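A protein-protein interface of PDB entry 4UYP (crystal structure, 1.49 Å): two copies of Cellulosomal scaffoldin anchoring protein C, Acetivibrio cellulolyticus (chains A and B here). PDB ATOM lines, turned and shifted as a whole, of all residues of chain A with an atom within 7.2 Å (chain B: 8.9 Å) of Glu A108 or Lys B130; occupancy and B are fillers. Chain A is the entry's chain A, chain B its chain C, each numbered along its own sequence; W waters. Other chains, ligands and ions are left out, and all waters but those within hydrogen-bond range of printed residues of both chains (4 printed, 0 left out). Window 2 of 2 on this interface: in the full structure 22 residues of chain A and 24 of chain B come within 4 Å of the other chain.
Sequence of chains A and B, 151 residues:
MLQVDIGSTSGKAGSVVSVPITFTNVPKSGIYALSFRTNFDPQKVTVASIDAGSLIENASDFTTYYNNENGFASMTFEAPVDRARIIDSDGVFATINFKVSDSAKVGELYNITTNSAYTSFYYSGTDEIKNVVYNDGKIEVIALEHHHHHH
No position is printed for both chains.
The backbone NH of Lys A105 is in hydrogen-bond range of the side-chain carboxylate of Glu A108 (3.1 Å). The side-chain carboxylate (OE1) of Glu A108 lies within hydrogen-bond range of the side-chain hydroxyl (OH) of Tyr A110 (2.6 Å). O of Lys A44 sits at hydrogen-bond distance from N of Ser A101 (2.9 Å). The backbone NH (N) of Gly A107 sits at hydrogen-bond distance from the backbone carbonyl oxygen (O) of Val A141, at 3.0 Å. The side-chain carboxylate (OD2) of Asp A41 lies within salt-bridge range of the side-chain amino group (NZ) of Lys A44. The backbone carbonyl oxygen (O) of Glu A108 sits at hydrogen-bond distance from the backbone NH (N) of Val A141.
The side-chain carboxylate of Glu A108 lies within salt-bridge range of the side-chain amino group of Lys B130, at 2.9 Å. ND2 of Asn A111 sits at hydrogen-bond distance from O of Val B132 (2.8 Å). The backbone carbonyl oxygen (O) of Lys B130 lies within hydrogen-bond range of the backbone NH (N) of Leu A109 (3.0 Å). NZ of Lys A44 is in salt-bridge range of OE2 of Glu B128 (2.7 Å).
Hydrophobic or aromatic side chains of chain B that line the printed part of chain A: Met B1 and Tyr B134. Among the printed residues, 8 pairs touch across the chains. Among the printed residues, Asp or Glu carboxylates within 4 Å of a Lys or Arg side-chain nitrogen of the other chain: Lys A44 with Glu B128 and Glu A108 with Lys B130.
Water W2 lies within hydrogen-bond range of the side-chain amide oxygen of Asn A111 and the backbone NH of Tyr B134. Water W4 lies within hydrogen-bond range of O of Leu A109 (2.7 Å) and N of Val B132 (3.0 Å). Water W3 lies within hydrogen-bond range of the side-chain amino group of Lys A44 (2.8 Å), the side-chain carboxylate of Asp A41 (2.8 Å) and the side-chain carboxylate of Glu B128 (3.3 Å). Water W1 lies within hydrogen-bond range of OE1 of Glu A108 (2.8 Å), NZ of Lys B130 (3.3 Å) and O of Ser A103 (3.4 Å).
Of the printed residues of chain B, Lys A44 touches Glu B128 (2.7 Å). Gly A107 touches just one residue of chain B: Asn B131. Of chain B, only Lys B130 (2.9 Å) comes within 4 Å of Glu A108. Printed residues of chain A within 4 Å of Met B1: Leu A109 (3.1 Å). Printed residues of chain A within 4 Å of Lys B130: Glu A108 (2.9 Å) and Leu A109 (3.0 Å). The nearest residue of chain B that does not touch Glu A108 is Asn B131 (4.6 Å).
Among the printed residues, merely in contact across the chains: Leu A109 with Met B1 (3.1 Å), Asn A111 with Tyr B134 (3.5 Å), Leu A109 with Asn B131 (3.6 Å) and Gly A107 with Asn B131 (3.8 Å).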
ATOM      1  N   ASP A  41      16.608   7.887  35.503  1.00  0.00           N
ATOM      2  CA  ASP A  41      17.122   6.522  35.858  1.00  0.00           C
ATOM      3  C   ASP A  41      18.655   6.575  35.708  1.00  0.00           C
ATOM      4  O   ASP A  41      19.095   6.816  34.571  1.00  0.00           O
ATOM      5  CB  ASP A  41      16.519   5.555  34.855  1.00  0.00           C
ATOM      6  CG  ASP A  41      17.053   4.128  35.043  1.00  0.00           C
ATOM      7  OD1 ASP A  41      18.079   3.904  35.734  1.00  0.00           O
ATOM      8  OD2 ASP A  41      16.375   3.232  34.487  1.00  0.00           O
ATOM      9  N   LYS A  44      20.663   4.921  32.996  1.00  0.00           N
ATOM     10  CA  LYS A  44      20.460   5.402  31.638  1.00  0.00           C
ATOM     11  C   LYS A  44      21.298   6.691  31.417  1.00  0.00           C
ATOM     12  O   LYS A  44      22.003   6.816  30.393  1.00  0.00           O
ATOM     13  CB  LYS A  44      18.956   5.645  31.346  1.00  0.00           C
ATOM     14  CG  LYS A  44      18.062   4.357  31.351  1.00  0.00           C
ATOM     15  CD  LYS A  44      16.552   4.679  31.463  1.00  0.00           C
ATOM     16  CE  LYS A  44      15.685   3.459  31.128  1.00  0.00           C
ATOM     17  NZ  LYS A  44      15.484   2.525  32.237  1.00  0.00           N
ATOM     18  N   SER A 101      24.649   6.777  29.284  1.00  0.00           N
ATOM     19  CA  SER A 101      25.362   5.496  29.468  1.00  0.00           C
ATOM     20  C   SER A 101      26.127   5.002  28.234  1.00  0.00           C
ATOM     21  O   SER A 101      25.542   5.048  27.109  1.00  0.00           O
ATOM     22  CB  SER A 101      24.345   4.406  29.766  1.00  0.00           C
ATOM     23  OG  SER A 101      25.057   3.265  30.155  1.00  0.00           O
ATOM     24  N   SER A 103      26.360   2.059  27.648  1.00  0.00           N
ATOM     25  CA  SER A 103      25.562   0.923  27.180  1.00  0.00           C
ATOM     26  C   SER A 103      24.222   1.222  26.534  1.00  0.00           C
ATOM     27  O   SER A 103      23.456   0.306  26.172  1.00  0.00           O
ATOM     28  CB  SER A 103      25.503  -0.125  28.232  1.00  0.00           C
ATOM     29  OG  SER A 103      24.849   0.346  29.367  1.00  0.00           O
ATOM     30  N   ALA A 104      23.879   2.499  26.326  1.00  0.00           N
ATOM     31  CA  ALA A 104      22.689   2.923  25.677  1.00  0.00           C
ATOM     32  C   ALA A 104      22.612   2.264  24.277  1.00  0.00           C
ATOM     33  O   ALA A 104      23.633   2.194  23.561  1.00  0.00           O
ATOM     34  CB  ALA A 104      22.702   4.460  25.557  1.00  0.00           C
ATOM     35  N   LYS A 105      21.412   1.963  23.854  1.00  0.00           N
ATOM     36  CA  LYS A 105      21.172   1.443  22.488  1.00  0.00           C
ATOM     37  C   LYS A 105      20.286   2.385  21.739  1.00  0.00           C
ATOM     38  O   LYS A 105      19.319   2.992  22.284  1.00  0.00           O
ATOM     39  CB  LYS A 105      20.522   0.038  22.519  1.00  0.00           C
ATOM     40  CG  LYS A 105      21.185  -0.897  23.511  1.00  0.00           C
ATOM     41  CD  LYS A 105      21.575  -2.279  22.980  1.00  0.00           C
ATOM     42  CE  LYS A 105      20.524  -2.839  22.019  1.00  0.00           C
ATOM     43  NZ  LYS A 105      20.692  -4.292  21.704  1.00  0.00           N
ATOM     44  N   VAL A 106      20.525   2.439  20.430  1.00  0.00           N
ATOM     45  CA  VAL A 106      19.750   3.240  19.568  1.00  0.00           C
ATOM     46  C   VAL A 106      18.230   2.944  19.710  1.00  0.00           C
ATOM     47  O   VAL A 106      17.812   1.769  19.755  1.00  0.00           O
ATOM     48  CB  VAL A 106      20.189   3.021  18.090  1.00  0.00           C
ATOM     49  CG1 VAL A 106      19.383   3.900  17.158  1.00  0.00           C
ATOM     50  CG2 VAL A 106      21.662   3.367  17.922  1.00  0.00           C
ATOM     51  N   GLY A 107      17.411   4.007  19.779  1.00  0.00           N
ATOM     52  CA  GLY A 107      15.958   4.012  20.030  1.00  0.00           C
ATOM     53  C   GLY A 107      15.420   3.988  21.438  1.00  0.00           C
ATOM     54  O   GLY A 107      14.210   4.103  21.677  1.00  0.00           O
ATOM     55  N   GLU A 108      16.326   3.890  22.417  1.00  0.00           N
ATOM     56  CA  GLU A 108      15.929   3.951  23.817  1.00  0.00           C
ATOM     57  C   GLU A 108      15.527   5.357  24.108  1.00  0.00           C
ATOM     58  O   GLU A 108      16.042   6.259  23.440  1.00  0.00           O
ATOM     59  CB  GLU A 108      17.049   3.457  24.638  1.00  0.00           C
ATOM     60  CG  GLU A 108      17.147   1.896  24.465  1.00  0.00           C
ATOM     61  CD  GLU A 108      18.205   1.255  25.285  1.00  0.00           C
ATOM     62  OE1 GLU A 108      19.072   1.951  25.896  1.00  0.00           O
ATOM     63  OE2 GLU A 108      18.269  -0.009  25.313  1.00  0.00           O
ATOM     64  N   LEU A 109      14.592   5.494  25.062  1.00  0.00           N
ATOM     65  CA  LEU A 109      14.039   6.822  25.465  1.00  0.00           C
ATOM     66  C   LEU A 109      14.172   6.923  26.948  1.00  0.00           C
ATOM     67  O   LEU A 109      13.662   6.084  27.671  1.00  0.00           O
ATOM     68  CB  LEU A 109      12.571   6.935  25.083  1.00  0.00           C
ATOM     69  CG  LEU A 109      12.448   6.826  23.608  1.00  0.00           C
ATOM     70  CD1 LEU A 109      10.913   6.729  23.379  1.00  0.00           C
ATOM     71  CD2 LEU A 109      13.013   8.020  22.852  1.00  0.00           C
ATOM     72  N   TYR A 110      14.835   8.010  27.434  1.00  0.00           N
ATOM     73  CA  TYR A 110      15.117   8.145  28.839  1.00  0.00           C
ATOM     74  C   TYR A 110      14.341   9.365  29.282  1.00  0.00           C
ATOM     75  O   TYR A 110      14.605  10.502  28.816  1.00  0.00           O
ATOM     76  CB  TYR A 110      16.577   8.308  29.095  1.00  0.00           C
ATOM     77  CG  TYR A 110      17.433   7.218  28.513  1.00  0.00           C
ATOM     78  CD1 TYR A 110      16.910   5.895  28.390  1.00  0.00           C
ATOM     79  CD2 TYR A 110      18.678   7.504  27.999  1.00  0.00           C
ATOM     80  CE1 TYR A 110      17.708   4.888  27.871  1.00  0.00           C
ATOM     81  CE2 TYR A 110      19.513   6.488  27.497  1.00  0.00           C
ATOM     82  CZ  TYR A 110      18.978   5.194  27.421  1.00  0.00           C
ATOM     83  OH  TYR A 110      19.787   4.202  26.890  1.00  0.00           O
ATOM     84  N   ASN A 111      13.349   9.144  30.092  1.00  0.00           N
ATOM     85  CA  ASN A 111      12.483  10.278  30.508  1.00  0.00           C
ATOM     86  C   ASN A 111      13.137  11.044  31.662  1.00  0.00           C
ATOM     87  O   ASN A 111      13.654  10.491  32.621  1.00  0.00           O
ATOM     88  CB  ASN A 111      11.168   9.669  31.048  1.00  0.00           C
ATOM     89  CG  ASN A 111      10.289   9.074  29.922  1.00  0.00           C
ATOM     90  OD1 ASN A 111       9.766   9.855  29.120  1.00  0.00           O
ATOM     91  ND2 ASN A 111      10.249   7.746  29.817  1.00  0.00           N
ATOM     92  N   ILE A 139      15.453  12.056  26.505  1.00  0.00           N
ATOM     93  CA  ILE A 139      16.699  11.931  25.754  1.00  0.00           C
ATOM     94  C   ILE A 139      16.570  10.655  24.893  1.00  0.00           C
ATOM     95  O   ILE A 139      16.354   9.602  25.435  1.00  0.00           O
ATOM     96  CB  ILE A 139      17.931  11.803  26.670  1.00  0.00           C
ATOM     97  CG1 ILE A 139      18.091  13.076  27.532  1.00  0.00           C
ATOM     98  CG2 ILE A 139      19.190  11.468  25.847  1.00  0.00           C
ATOM     99  CD1 ILE A 139      19.088  12.907  28.688  1.00  0.00           C
ATOM    100  N   GLU A 140      16.695  10.857  23.627  1.00  0.00           N
ATOM    101  CA  GLU A 140      16.657   9.722  22.658  1.00  0.00           C
ATOM    102  C   GLU A 140      18.044   9.329  22.261  1.00  0.00           C
ATOM    103  O   GLU A 140      18.877  10.153  21.926  1.00  0.00           O
ATOM    104  CB  GLU A 140      15.931  10.183  21.407  1.00  0.00           C
ATOM    105  CG  GLU A 140      15.811   9.046  20.350  1.00  0.00           C
ATOM    106  CD  GLU A 140      15.108   9.526  19.066  1.00  0.00           C
ATOM    107  OE1 GLU A 140      14.243  10.434  19.163  1.00  0.00           O
ATOM    108  OE2 GLU A 140      15.416   9.000  17.962  1.00  0.00           O
ATOM    109  N   VAL A 141      18.290   8.022  22.255  1.00  0.00           N
ATOM    110  CA  VAL A 141      19.593   7.563  21.820  1.00  0.00           C
ATOM    111  C   VAL A 141      19.635   7.359  20.319  1.00  0.00           C
ATOM    112  O   VAL A 141      18.735   6.645  19.802  1.00  0.00           O
ATOM    113  CB  VAL A 141      19.934   6.219  22.525  1.00  0.00           C
ATOM    114  CG1 VAL A 141      21.342   5.768  22.169  1.00  0.00           C
ATOM    115  CG2 VAL A 141      19.800   6.349  24.063  1.00  0.00           C
ATOM    116  N   ILE A 142      20.639   7.955  19.717  1.00  0.00           N
ATOM    117  CA  ILE A 142      20.858   7.890  18.292  1.00  0.00           C
ATOM    118  C   ILE A 142      22.166   7.224  17.961  1.00  0.00           C
ATOM    119  O   ILE A 142      23.046   7.048  18.774  1.00  0.00           O
ATOM    120  CB  ILE A 142      20.818   9.266  17.656  1.00  0.00           C
ATOM    121  CG1 ILE A 142      21.906  10.131  18.290  1.00  0.00           C
ATOM    122  CG2 ILE A 142      19.419   9.836  17.822  1.00  0.00           C
ATOM    123  CD1 ILE A 142      22.256  11.352  17.544  1.00  0.00           C
ATOM    124  N   MET B   1       5.365   2.606  20.903  1.00  0.00           N
ATOM    125  CA  MET B   1       5.955   2.038  22.150  1.00  0.00           C
ATOM    126  C   MET B   1       4.936   2.148  23.268  1.00  0.00           C
ATOM    127  O   MET B   1       3.889   2.778  23.075  1.00  0.00           O
ATOM    128  CB  MET B   1       7.183   2.801  22.509  1.00  0.00           C
ATOM    129  CG  MET B   1       6.948   4.227  22.915  1.00  0.00           C
ATOM    130  SD  MET B   1       8.426   5.092  22.448  1.00  0.00           S
ATOM    131  CE  MET B   1       8.149   5.090  20.659  1.00  0.00           C
ATOM    132  N   LEU B   2       5.226   1.426  24.347  1.00  0.00           N
ATOM    133  CA  LEU B   2       4.319   1.466  25.527  1.00  0.00           C
ATOM    134  C   LEU B   2       4.181   2.910  26.002  1.00  0.00           C
ATOM    135  O   LEU B   2       5.194   3.608  26.142  1.00  0.00           O
ATOM    136  CB  LEU B   2       5.025   0.653  26.589  1.00  0.00           C
ATOM    137  CG  LEU B   2       4.310   0.608  27.949  1.00  0.00           C
ATOM    138  CD1 LEU B   2       2.918   0.017  27.895  1.00  0.00           C
ATOM    139  CD2 LEU B   2       5.163  -0.157  28.999  1.00  0.00           C
ATOM    140  N   SER B 120       9.821   1.691  36.300  1.00  0.00           N
ATOM    141  CA  SER B 120      10.545   0.867  35.273  1.00  0.00           C
ATOM    142  C   SER B 120       9.621  -0.264  34.907  1.00  0.00           C
ATOM    143  O   SER B 120       8.754  -0.692  35.675  1.00  0.00           O
ATOM    144  CB  SER B 120      11.852   0.235  35.769  1.00  0.00           C
ATOM    145  OG  SER B 120      11.695  -0.782  36.765  1.00  0.00           O
ATOM    146  N   PHE B 121       9.816  -0.815  33.717  1.00  0.00           N
ATOM    147  CA  PHE B 121       8.963  -1.870  33.122  1.00  0.00           C
ATOM    148  C   PHE B 121       9.836  -2.957  32.524  1.00  0.00           C
ATOM    149  O   PHE B 121      10.849  -2.613  31.882  1.00  0.00           O
ATOM    150  CB  PHE B 121       8.101  -1.315  32.033  1.00  0.00           C
ATOM    151  CG  PHE B 121       7.026  -0.353  32.513  1.00  0.00           C
ATOM    152  CD1 PHE B 121       7.353   0.965  32.816  1.00  0.00           C
ATOM    153  CD2 PHE B 121       5.759  -0.761  32.597  1.00  0.00           C
ATOM    154  CE1 PHE B 121       6.281   1.805  33.269  1.00  0.00           C
ATOM    155  CE2 PHE B 121       4.716   0.069  33.009  1.00  0.00           C
ATOM    156  CZ  PHE B 121       5.023   1.339  33.385  1.00  0.00           C
ATOM    157  N   TYR B 122       9.468  -4.197  32.782  1.00  0.00           N
ATOM    158  CA  TYR B 122      10.331  -5.372  32.354  1.00  0.00           C
ATOM    159  C   TYR B 122       9.492  -6.382  31.585  1.00  0.00           C
ATOM    160  O   TYR B 122       8.423  -6.787  32.012  1.00  0.00           O
ATOM    161  CB  TYR B 122      10.947  -6.025  33.546  1.00  0.00           C
ATOM    162  CG  TYR B 122      12.137  -5.238  34.100  1.00  0.00           C
ATOM    163  CD1 TYR B 122      11.959  -4.102  34.934  1.00  0.00           C
ATOM    164  CD2 TYR B 122      13.433  -5.553  33.699  1.00  0.00           C
ATOM    165  CE1 TYR B 122      13.052  -3.378  35.331  1.00  0.00           C
ATOM    166  CE2 TYR B 122      14.503  -4.782  34.084  1.00  0.00           C
ATOM    167  CZ  TYR B 122      14.321  -3.717  34.914  1.00  0.00           C
ATOM    168  OH  TYR B 122      15.389  -2.902  35.321  1.00  0.00           O
ATOM    169  N   TYR B 123      10.036  -6.853  30.468  1.00  0.00           N
ATOM    170  CA  TYR B 123       9.476  -8.027  29.753  1.00  0.00           C
ATOM    171  C   TYR B 123       9.807  -9.348  30.480  1.00  0.00           C
ATOM    172  O   TYR B 123       9.034 -10.281  30.324  1.00  0.00           O
ATOM    173  CB  TYR B 123      10.298  -8.143  28.450  1.00  0.00           C
ATOM    174  CG  TYR B 123      10.052  -7.060  27.419  1.00  0.00           C
ATOM    175  CD1 TYR B 123       8.788  -6.863  26.826  1.00  0.00           C
ATOM    176  CD2 TYR B 123      11.140  -6.248  27.007  1.00  0.00           C
ATOM    177  CE1 TYR B 123       8.604  -5.894  25.870  1.00  0.00           C
ATOM    178  CE2 TYR B 123      10.913  -5.277  25.991  1.00  0.00           C
ATOM    179  CZ  TYR B 123       9.664  -5.147  25.452  1.00  0.00           C
ATOM    180  OH  TYR B 123       9.420  -4.156  24.481  1.00  0.00           O
ATOM    181  N   THR B 126      15.273 -10.070  33.348  1.00  0.00           N
ATOM    182  CA  THR B 126      16.476  -9.390  32.949  1.00  0.00           C
ATOM    183  C   THR B 126      16.324  -8.513  31.761  1.00  0.00           C
ATOM    184  O   THR B 126      17.369  -8.008  31.203  1.00  0.00           O
ATOM    185  CB  THR B 126      17.637 -10.410  32.664  1.00  0.00           C
ATOM    186  OG1 THR B 126      17.133 -11.348  31.707  1.00  0.00           O
ATOM    187  CG2 THR B 126      17.995 -11.144  33.937  1.00  0.00           C
ATOM    188  N   ASP B 127      15.191  -8.445  31.158  1.00  0.00           N
ATOM    189  CA  ASP B 127      15.029  -7.663  29.947  1.00  0.00           C
ATOM    190  C   ASP B 127      14.038  -6.552  30.157  1.00  0.00           C
ATOM    191  O   ASP B 127      12.809  -6.753  30.295  1.00  0.00           O
ATOM    192  CB  ASP B 127      14.502  -8.538  28.795  1.00  0.00           C
ATOM    193  CG  ASP B 127      15.397  -9.656  28.443  1.00  0.00           C
ATOM    194  OD1 ASP B 127      16.513  -9.409  28.019  1.00  0.00           O
ATOM    195  OD2 ASP B 127      14.928 -10.790  28.558  1.00  0.00           O
ATOM    196  N   GLU B 128      14.569  -5.331  30.143  1.00  0.00           N
ATOM    197  CA  GLU B 128      13.830  -4.115  30.485  1.00  0.00           C
ATOM    198  C   GLU B 128      13.180  -3.571  29.218  1.00  0.00           C
ATOM    199  O   GLU B 128      13.798  -3.596  28.128  1.00  0.00           O
ATOM    200  CB  GLU B 128      14.782  -3.044  31.120  1.00  0.00           C
ATOM    201  CG  GLU B 128      14.013  -1.807  31.618  1.00  0.00           C
ATOM    202  CD  GLU B 128      14.957  -0.772  32.231  1.00  0.00           C
ATOM    203  OE1 GLU B 128      16.201  -0.945  32.215  1.00  0.00           O
ATOM    204  OE2 GLU B 128      14.406   0.154  32.826  1.00  0.00           O
ATOM    205  N   ILE B 129      11.993  -2.977  29.355  1.00  0.00           N
ATOM    206  CA  ILE B 129      11.376  -2.156  28.313  1.00  0.00           C
ATOM    207  C   ILE B 129      11.986  -0.768  28.411  1.00  0.00           C
ATOM    208  O   ILE B 129      11.757   0.004  29.347  1.00  0.00           O
ATOM    209  CB  ILE B 129       9.817  -2.110  28.501  1.00  0.00           C
ATOM    210  CG1 ILE B 129       9.250  -3.515  28.732  1.00  0.00           C
ATOM    211  CG2 ILE B 129       9.200  -1.413  27.263  1.00  0.00           C
ATOM    212  CD1 ILE B 129       7.694  -3.563  28.724  1.00  0.00           C
ATOM    213  N   LYS B 130      12.826  -0.392  27.452  1.00  0.00           N
ATOM    214  CA  LYS B 130      13.609   0.833  27.623  1.00  0.00           C
ATOM    215  C   LYS B 130      13.167   1.971  26.697  1.00  0.00           C
ATOM    216  O   LYS B 130      13.969   2.970  26.527  1.00  0.00           O
ATOM    217  CB  LYS B 130      15.128   0.577  27.578  1.00  0.00           C
ATOM    218  CG  LYS B 130      15.650  -0.255  28.730  1.00  0.00           C
ATOM    219  CD  LYS B 130      17.075  -0.708  28.432  1.00  0.00           C
ATOM    220  CE  LYS B 130      17.136  -2.013  27.698  1.00  0.00           C
ATOM    221  NZ  LYS B 130      18.564  -2.114  27.353  1.00  0.00           N
ATOM    222  N   ASN B 131      11.981   1.839  26.079  1.00  0.00           N
ATOM    223  CA  ASN B 131      11.411   2.970  25.404  1.00  0.00           C
ATOM    224  C   ASN B 131       9.982   3.356  25.735  1.00  0.00           C
ATOM    225  O   ASN B 131       9.276   3.911  24.904  1.00  0.00           O
ATOM    226  CB  ASN B 131      11.450   2.727  23.886  1.00  0.00           C
ATOM    227  CG  ASN B 131      10.730   1.503  23.499  1.00  0.00           C
ATOM    228  OD1 ASN B 131      10.355   0.679  24.356  1.00  0.00           O
ATOM    229  ND2 ASN B 131      10.514   1.330  22.198  1.00  0.00           N
ATOM    230  N   VAL B 132       9.689   3.376  26.993  1.00  0.00           N
ATOM    231  CA  VAL B 132       8.331   3.722  27.433  1.00  0.00           C
ATOM    232  C   VAL B 132       8.179   5.230  27.529  1.00  0.00           C
ATOM    233  O   VAL B 132       9.197   5.942  27.898  1.00  0.00           O
ATOM    234  CB  VAL B 132       8.176   3.181  28.865  1.00  0.00           C
ATOM    235  CG1 VAL B 132       6.756   3.382  29.396  1.00  0.00           C
ATOM    236  CG2 VAL B 132       8.524   1.765  28.936  1.00  0.00           C
ATOM    237  N   VAL B 133       7.056   5.698  27.121  1.00  0.00           N
ATOM    238  CA  VAL B 133       6.643   7.136  27.142  1.00  0.00           C
ATOM    239  C   VAL B 133       5.648   7.381  28.295  1.00  0.00           C
ATOM    240  O   VAL B 133       4.812   6.567  28.579  1.00  0.00           O
ATOM    241  CB  VAL B 133       6.070   7.593  25.781  1.00  0.00           C
ATOM    242  CG1 VAL B 133       5.268   6.537  25.097  1.00  0.00           C
ATOM    243  CG2 VAL B 133       5.247   8.890  25.840  1.00  0.00           C
ATOM    244  N   TYR B 134       5.674   8.576  28.826  1.00  0.00           N
ATOM    245  CA  TYR B 134       4.729   8.879  29.898  1.00  0.00           C
ATOM    246  C   TYR B 134       4.030  10.169  29.607  1.00  0.00           C
ATOM    247  O   TYR B 134       4.641  11.085  28.992  1.00  0.00           O
ATOM    248  CB  TYR B 134       5.502   9.229  31.113  1.00  0.00           C
ATOM    249  CG  TYR B 134       6.561   8.417  31.631  1.00  0.00           C
ATOM    250  CD1 TYR B 134       6.577   7.027  31.513  1.00  0.00           C
ATOM    251  CD2 TYR B 134       7.578   9.029  32.314  1.00  0.00           C
ATOM    252  CE1 TYR B 134       7.595   6.263  32.015  1.00  0.00           C
ATOM    253  CE2 TYR B 134       8.574   8.306  32.892  1.00  0.00           C
ATOM    254  CZ  TYR B 134       8.586   6.980  32.756  1.00  0.00           C
ATOM    255  OH  TYR B 134       9.589   6.314  33.322  1.00  0.00           O
HETATM  256  O   HOH W   1      20.466   0.528  27.815  1.00  0.00           O
HETATM  257  O   HOH W   2       7.646  10.309  27.635  1.00  0.00           O
HETATM  258  O   HOH W   3      13.635   3.049  34.212  1.00  0.00           O
HETATM  259  O   HOH W   4      11.735   4.591  28.750  1.00  0.00           O
